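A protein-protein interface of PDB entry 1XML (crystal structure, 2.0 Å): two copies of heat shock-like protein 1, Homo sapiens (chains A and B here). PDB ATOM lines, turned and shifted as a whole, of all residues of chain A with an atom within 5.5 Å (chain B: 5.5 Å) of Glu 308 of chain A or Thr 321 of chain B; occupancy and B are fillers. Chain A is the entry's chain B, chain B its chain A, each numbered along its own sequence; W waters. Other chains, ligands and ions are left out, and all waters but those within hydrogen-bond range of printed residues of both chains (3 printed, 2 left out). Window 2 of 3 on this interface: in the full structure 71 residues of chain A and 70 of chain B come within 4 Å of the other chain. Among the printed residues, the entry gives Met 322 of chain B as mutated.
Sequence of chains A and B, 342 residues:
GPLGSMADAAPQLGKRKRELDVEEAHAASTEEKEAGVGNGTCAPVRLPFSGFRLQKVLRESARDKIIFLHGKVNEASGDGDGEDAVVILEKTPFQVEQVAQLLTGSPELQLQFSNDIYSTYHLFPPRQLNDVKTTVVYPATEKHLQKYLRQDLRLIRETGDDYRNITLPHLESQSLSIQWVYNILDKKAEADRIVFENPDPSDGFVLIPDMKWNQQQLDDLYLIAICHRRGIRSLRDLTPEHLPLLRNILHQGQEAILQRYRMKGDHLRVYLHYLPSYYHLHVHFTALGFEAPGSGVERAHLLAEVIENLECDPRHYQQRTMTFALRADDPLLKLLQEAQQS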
ATOM      1  N   LEU A 303      29.152  -3.498  30.551  1.00  0.00           N
ATOM      2  CA  LEU A 303      28.841  -4.632  29.678  1.00  0.00           C
ATOM      3  C   LEU A 303      27.630  -4.383  28.790  1.00  0.00           C
ATOM      4  O   LEU A 303      27.630  -4.756  27.615  1.00  0.00           O
ATOM      5  CB  LEU A 303      28.572  -5.917  30.487  1.00  0.00           C
ATOM      6  CG  LEU A 303      29.144  -7.242  29.992  1.00  0.00           C
ATOM      7  CD1 LEU A 303      28.405  -8.432  30.581  1.00  0.00           C
ATOM      8  CD2 LEU A 303      29.294  -7.371  28.489  1.00  0.00           C
ATOM      9  N   ALA A 304      26.586  -3.801  29.369  1.00  0.00           N
ATOM     10  CA  ALA A 304      25.388  -3.469  28.624  1.00  0.00           C
ATOM     11  C   ALA A 304      25.707  -2.569  27.418  1.00  0.00           C
ATOM     12  O   ALA A 304      25.106  -2.721  26.360  1.00  0.00           O
ATOM     13  CB  ALA A 304      24.343  -2.821  29.544  1.00  0.00           C
ATOM     14  N   GLU A 305      26.662  -1.656  27.584  1.00  0.00           N
ATOM     15  CA  GLU A 305      27.067  -0.734  26.528  1.00  0.00           C
ATOM     16  C   GLU A 305      27.963  -1.413  25.500  1.00  0.00           C
ATOM     17  O   GLU A 305      27.868  -1.109  24.329  1.00  0.00           O
ATOM     18  CB  GLU A 305      27.817   0.464  27.105  1.00  0.00           C
ATOM     19  CG  GLU A 305      26.978   1.323  28.022  1.00  0.00           C
ATOM     20  CD  GLU A 305      27.608   2.682  28.294  1.00  0.00           C
ATOM     21  OE1 GLU A 305      26.865   3.611  28.671  1.00  0.00           O
ATOM     22  OE2 GLU A 305      28.844   2.820  28.139  1.00  0.00           O
ATOM     23  N   VAL A 306      28.829  -2.319  25.951  1.00  0.00           N
ATOM     24  CA  VAL A 306      29.658  -3.124  25.046  1.00  0.00           C
ATOM     25  C   VAL A 306      28.748  -3.884  24.081  1.00  0.00           C
ATOM     26  O   VAL A 306      28.976  -3.891  22.865  1.00  0.00           O
ATOM     27  CB  VAL A 306      30.589  -4.106  25.813  1.00  0.00           C
ATOM     28  CG1 VAL A 306      31.306  -5.050  24.853  1.00  0.00           C
ATOM     29  CG2 VAL A 306      31.637  -3.323  26.608  1.00  0.00           C
ATOM     30  N   ILE A 307      27.692  -4.477  24.629  1.00  0.00           N
ATOM     31  CA  ILE A 307      26.736  -5.239  23.840  1.00  0.00           C
ATOM     32  C   ILE A 307      26.049  -4.357  22.794  1.00  0.00           C
ATOM     33  O   ILE A 307      25.983  -4.704  21.599  1.00  0.00           O
ATOM     34  CB  ILE A 307      25.713  -5.923  24.785  1.00  0.00           C
ATOM     35  CG1 ILE A 307      26.408  -7.050  25.549  1.00  0.00           C
ATOM     36  CG2 ILE A 307      24.477  -6.433  24.028  1.00  0.00           C
ATOM     37  CD1 ILE A 307      25.583  -7.621  26.670  1.00  0.00           C
ATOM     38  N   GLU A 308      25.571  -3.198  23.230  1.00  0.00           N
ATOM     39  CA  GLU A 308      24.867  -2.298  22.326  1.00  0.00           C
ATOM     40  C   GLU A 308      25.781  -1.712  21.246  1.00  0.00           C
ATOM     41  O   GLU A 308      25.383  -1.616  20.087  1.00  0.00           O
ATOM     42  CB  GLU A 308      24.128  -1.228  23.127  1.00  0.00           C
ATOM     43  CG  GLU A 308      22.939  -1.849  23.841  1.00  0.00           C
ATOM     44  CD  GLU A 308      22.156  -0.877  24.689  1.00  0.00           C
ATOM     45  OE1 GLU A 308      22.640   0.250  24.908  1.00  0.00           O
ATOM     46  OE2 GLU A 308      21.050  -1.260  25.136  1.00  0.00           O
ATOM     47  N   ASN A 309      27.013  -1.379  21.610  1.00  0.00           N
ATOM     48  CA  ASN A 309      28.050  -1.011  20.640  1.00  0.00           C
ATOM     49  C   ASN A 309      28.242  -2.062  19.551  1.00  0.00           C
ATOM     50  O   ASN A 309      28.313  -1.727  18.376  1.00  0.00           O
ATOM     51  CB  ASN A 309      29.393  -0.742  21.351  1.00  0.00           C
ATOM     52  CG  ASN A 309      29.400   0.583  22.104  1.00  0.00           C
ATOM     53  OD1 ASN A 309      28.581   1.440  21.846  1.00  0.00           O
ATOM     54  ND2 ASN A 309      30.341   0.749  23.027  1.00  0.00           N
ATOM     55  N   LEU A 310      28.320  -3.328  19.944  1.00  0.00           N
ATOM     56  CA  LEU A 310      28.532  -4.417  18.996  1.00  0.00           C
ATOM     57  C   LEU A 310      27.331  -4.588  18.074  1.00  0.00           C
ATOM     58  O   LEU A 310      27.487  -4.925  16.892  1.00  0.00           O
ATOM     59  CB  LEU A 310      28.791  -5.730  19.735  1.00  0.00           C
ATOM     60  CG  LEU A 310      30.197  -5.909  20.316  1.00  0.00           C
ATOM     61  CD1 LEU A 310      30.238  -7.084  21.268  1.00  0.00           C
ATOM     62  CD2 LEU A 310      31.207  -6.102  19.185  1.00  0.00           C
ATOM     63  N   GLU A 311      26.140  -4.358  18.617  1.00  0.00           N
ATOM     64  CA  GLU A 311      24.910  -4.439  17.841  1.00  0.00           C
ATOM     65  C   GLU A 311      24.810  -3.284  16.856  1.00  0.00           C
ATOM     66  O   GLU A 311      24.299  -3.472  15.756  1.00  0.00           O
ATOM     67  CB  GLU A 311      23.680  -4.469  18.762  1.00  0.00           C
ATOM     68  CG  GLU A 311      23.551  -5.740  19.606  1.00  0.00           C
ATOM     69  CD  GLU A 311      22.516  -5.631  20.737  1.00  0.00           C
ATOM     70  OE1 GLU A 311      22.165  -4.503  21.157  1.00  0.00           O
ATOM     71  OE2 GLU A 311      22.050  -6.681  21.234  1.00  0.00           O
ATOM     72  N   CYS A 312      25.300  -2.100  17.246  1.00  0.00           N
ATOM     73  CA  CYS A 312      25.198  -0.882  16.434  1.00  0.00           C
ATOM     74  C   CYS A 312      26.304  -0.761  15.391  1.00  0.00           C
ATOM     75  O   CYS A 312      26.103  -0.156  14.340  1.00  0.00           O
ATOM     76  CB  CYS A 312      25.250   0.382  17.318  1.00  0.00           C
ATOM     77  SG  CYS A 312      23.755   0.681  18.260  1.00  0.00           S
ATOM     78  N   ASP A 313      27.470  -1.313  15.697  1.00  0.00           N
ATOM     79  CA  ASP A 313      28.644  -1.193  14.841  1.00  0.00           C
ATOM     80  C   ASP A 313      29.531  -2.413  15.076  1.00  0.00           C
ATOM     81  O   ASP A 313      30.282  -2.450  16.048  1.00  0.00           O
ATOM     82  CB  ASP A 313      29.399   0.098  15.149  1.00  0.00           C
ATOM     83  CG  ASP A 313      30.763   0.162  14.476  1.00  0.00           C
ATOM     84  OD1 ASP A 313      31.036  -0.609  13.513  1.00  0.00           O
ATOM     85  OD2 ASP A 313      31.643   0.952  14.864  1.00  0.00           O
ATOM     86  N   ARG B 157      18.928   2.823  33.157  1.00  0.00           N
ATOM     87  CA  ARG B 157      19.301   2.940  31.754  1.00  0.00           C
ATOM     88  C   ARG B 157      18.225   3.730  31.025  1.00  0.00           C
ATOM     89  O   ARG B 157      17.126   3.263  30.867  1.00  0.00           O
ATOM     90  CB  ARG B 157      19.457   1.554  31.142  1.00  0.00           C
ATOM     91  CG  ARG B 157      20.473   0.715  31.879  1.00  0.00           C
ATOM     92  CD  ARG B 157      21.155  -0.331  31.037  1.00  0.00           C
ATOM     93  NE  ARG B 157      22.042   0.266  30.039  1.00  0.00           N
ATOM     94  CZ  ARG B 157      22.008   0.010  28.733  1.00  0.00           C
ATOM     95  NH1 ARG B 157      21.144  -0.851  28.219  1.00  0.00           N
ATOM     96  NH2 ARG B 157      22.877   0.608  27.931  1.00  0.00           N
ATOM     97  N   GLU B 158      18.555   4.942  30.611  1.00  0.00           N
ATOM     98  CA  GLU B 158      17.614   5.854  29.956  1.00  0.00           C
ATOM     99  C   GLU B 158      17.770   5.786  28.442  1.00  0.00           C
ATOM    100  O   GLU B 158      18.802   6.183  27.896  1.00  0.00           O
ATOM    101  CB  GLU B 158      17.900   7.271  30.478  1.00  0.00           C
ATOM    102  CG  GLU B 158      17.158   8.415  29.801  1.00  0.00           C
ATOM    103  CD  GLU B 158      17.934   9.715  29.872  1.00  0.00           C
ATOM    104  OE1 GLU B 158      17.498  10.630  30.586  1.00  0.00           O
ATOM    105  OE2 GLU B 158      18.999   9.819  29.226  1.00  0.00           O
ATOM    106  N   THR B 159      16.768   5.248  27.752  1.00  0.00           N
ATOM    107  CA  THR B 159      16.786   5.243  26.289  1.00  0.00           C
ATOM    108  C   THR B 159      16.557   6.662  25.770  1.00  0.00           C
ATOM    109  O   THR B 159      16.151   7.551  26.519  1.00  0.00           O
ATOM    110  CB  THR B 159      15.720   4.303  25.724  1.00  0.00           C
ATOM    111  OG1 THR B 159      14.422   4.777  26.093  1.00  0.00           O
ATOM    112  CG2 THR B 159      15.795   2.920  26.360  1.00  0.00           C
ATOM    113  N   GLY B 160      16.835   6.870  24.488  1.00  0.00           N
ATOM    114  CA  GLY B 160      16.561   8.137  23.827  1.00  0.00           C
ATOM    115  C   GLY B 160      15.107   8.561  23.992  1.00  0.00           C
ATOM    116  O   GLY B 160      14.821   9.733  24.259  1.00  0.00           O
ATOM    117  N   ARG B 236      22.943  15.146  26.308  1.00  0.00           N
ATOM    118  CA  ARG B 236      21.782  14.771  25.523  1.00  0.00           C
ATOM    119  C   ARG B 236      21.445  15.720  24.396  1.00  0.00           C
ATOM    120  O   ARG B 236      20.787  15.322  23.441  1.00  0.00           O
ATOM    121  CB  ARG B 236      20.553  14.618  26.424  1.00  0.00           C
ATOM    122  CG  ARG B 236      20.444  13.252  27.041  1.00  0.00           C
ATOM    123  CD  ARG B 236      20.075  12.189  26.019  1.00  0.00           C
ATOM    124  NE  ARG B 236      19.758  10.930  26.675  1.00  0.00           N
ATOM    125  CZ  ARG B 236      19.728   9.757  26.058  1.00  0.00           C
ATOM    126  NH1 ARG B 236      20.023   9.656  24.768  1.00  0.00           N
ATOM    127  NH2 ARG B 236      19.434   8.662  26.740  1.00  0.00           N
ATOM    128  N   GLN B 319      19.841   9.147  20.254  1.00  0.00           N
ATOM    129  CA  GLN B 319      19.277   7.819  19.984  1.00  0.00           C
ATOM    130  C   GLN B 319      19.720   6.755  20.994  1.00  0.00           C
ATOM    131  O   GLN B 319      18.952   5.884  21.351  1.00  0.00           O
ATOM    132  CB  GLN B 319      19.624   7.368  18.566  1.00  0.00           C
ATOM    133  CG  GLN B 319      18.977   8.213  17.487  1.00  0.00           C
ATOM    134  CD  GLN B 319      19.110   7.597  16.107  1.00  0.00           C
ATOM    135  OE1 GLN B 319      20.145   6.998  15.776  1.00  0.00           O
ATOM    136  NE2 GLN B 319      18.068   7.744  15.292  1.00  0.00           N
ATOM    137  N   ARG B 320      20.954   6.841  21.464  1.00  0.00           N
ATOM    138  CA  ARG B 320      21.550   5.797  22.284  1.00  0.00           C
ATOM    139  C   ARG B 320      21.126   5.868  23.743  1.00  0.00           C
ATOM    140  O   ARG B 320      20.636   6.876  24.209  1.00  0.00           O
ATOM    141  CB  ARG B 320      23.071   5.865  22.181  1.00  0.00           C
ATOM    142  CG  ARG B 320      23.595   5.539  20.780  1.00  0.00           C
ATOM    143  CD  ARG B 320      23.233   4.134  20.270  1.00  0.00           C
ATOM    144  NE  ARG B 320      24.377   3.238  20.437  1.00  0.00           N
ATOM    145  CZ  ARG B 320      24.733   2.672  21.576  1.00  0.00           C
ATOM    146  NH1 ARG B 320      24.025   2.872  22.666  1.00  0.00           N
ATOM    147  NH2 ARG B 320      25.811   1.902  21.638  1.00  0.00           N
ATOM    148  N   THR B 321      21.327   4.765  24.447  1.00  0.00           N
ATOM    149  CA  THR B 321      20.894   4.619  25.819  1.00  0.00           C
ATOM    150  C   THR B 321      22.017   5.077  26.743  1.00  0.00           C
ATOM    151  O   THR B 321      23.185   4.717  26.551  1.00  0.00           O
ATOM    152  CB  THR B 321      20.527   3.152  26.090  1.00  0.00           C
ATOM    153  OG1 THR B 321      19.356   2.795  25.335  1.00  0.00           O
ATOM    154  CG2 THR B 321      20.148   2.924  27.571  1.00  0.00           C
ATOM    155  N   MET B 322      21.656   5.887  27.732  1.00  0.00           N
ATOM    156  CA  MET B 322      22.596   6.381  28.723  1.00  0.00           C
ATOM    157  C   MET B 322      22.366   5.661  30.055  1.00  0.00           C
ATOM    158  O   MET B 322      21.242   5.358  30.412  1.00  0.00           O
ATOM    159  CB  MET B 322      22.433   7.898  28.896  1.00  0.00           C
ATOM    160  CG  MET B 322      22.742   8.702  27.617  1.00  0.00           C
ATOM    161  SD  MET B 322      24.496   8.690  27.140  1.00  0.00           S
ATOM    162  CE  MET B 322      25.056   9.587  28.391  1.00  0.00           C
ATOM    163  N   THR B 323      23.439   5.409  30.794  1.00  0.00           N
ATOM    164  CA  THR B 323      23.351   4.732  32.083  1.00  0.00           C
ATOM    165  C   THR B 323      23.864   5.641  33.166  1.00  0.00           C
ATOM    166  O   THR B 323      24.942   6.198  33.038  1.00  0.00           O
ATOM    167  CB  THR B 323      24.195   3.458  32.077  1.00  0.00           C
ATOM    168  OG1 THR B 323      23.702   2.573  31.074  1.00  0.00           O
ATOM    169  CG2 THR B 323      24.021   2.670  33.399  1.00  0.00           C
HETATM  170  O   HOH W   1      24.413   2.068  25.371  1.00  0.00           O
HETATM  171  O   HOH W   2      26.211   5.885  29.672  1.00  0.00           O
HETATM  172  O   HOH W   3      19.014   0.244  25.393  1.00  0.00           O
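Of the printed residues of chain B, Glu 308 of chain A touches Arg 157 (3.1 Å), Arg 320 (3.6 Å) and Thr 321 (3.8 Å). Thr 321 of chain B touches just one residue of chain A: Glu 308 (3.8 Å). Of the printed residues of chain B, Cys 312 of chain A touches Arg 320. Printed residues of chain B within 4 Å of Asn 309 of chain A: Arg 320. Printed residues of chain B within 4 Å of Ala 304 of chain A: Arg 157 (3.8 Å). Of the printed residues of chain A, Arg 157 of chain B touches Ala 304 (3.8 Å) and Glu 308 (3.1 Å). The nearest printed residue of chain B that does not touch Glu 308 of chain A is Met 322 of chain B (6.4 Å). The nearest printed residue of chain B that does not touch Cys 312 of chain A is Gln 319 of chain B (7.7 Å).
Water W3 bridges the side-chain carboxylate (OE2) of Glu 308 of chain A (2.5 Å) and the side-chain hydroxyl (OG1) of Thr 321 of chain B (2.6 Å). Water W2 lies within hydrogen-bond range of OE1 of Glu 305 of chain A (2.6 Å) and N of Thr 323 of chain B (3.0 Å). Water W1 lies within hydrogen-bond range of the side-chain carboxylate (OE1) of Glu 308 of chain A, the guanidinium group (NH1) of Arg 320 of chain B, the backbone carbonyl oxygen (O) of Thr 321 of chain B and the guanidinium group (NH2) of Arg 157 of chain B.
No position is printed for both chains.
CZ of Arg 157 of chain B touches CB of Ala 304 of chain A, at 3.8 Å. Thr 321 of chain B touches Glu 308 of chain A.
O of Glu 305 of chain A sits close to ND2 of Asn 309 of chain A (3.4 Å). O of Glu 308 of chain A is in hydrogen-bond range of SG of Cys 312 of chain A (3.4 Å). The guanidinium group (NE) of Arg 157 of chain B sits at hydrogen-bond distance from the side-chain hydroxyl (OG1) of Thr 323 of chain B (3.0 Å). The guanidinium group (NH1) of Arg 236 of chain B lies within hydrogen-bond range of the backbone carbonyl oxygen (O) of Arg 320 of chain B, at 2.9 Å.
OE1 of Glu 308 of chain A lies within salt-bridge range of NH2 of Arg 157 of chain B. The guanidinium group (NH1) of Arg 320 of chain B is in salt-bridge range of the side-chain carboxylate (OE1) of Glu 308 of chain A, 3.7 Å away. The side-chain amide oxygen of Asn 309 of chain A is in hydrogen-bond range of the guanidinium group of Arg 320 of chain B (2.8 Å). The guanidinium group of Arg 320 of chain B is in hydrogen-bond range of the side-chain sulfur of Cys 312 of chain A, at 3.4 Å.
Hydrophobic or aromatic side chains of chain A within 4 Å of the printed part of chain B: Ala 304. Among the printed residues, Asp or Glu carboxylates within 4 Å of a Lys or Arg side-chain nitrogen of the other chain: Glu 308 of chain A with Arg 157 of chain B and Glu 308 of chain A with Arg 320 of chain B.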
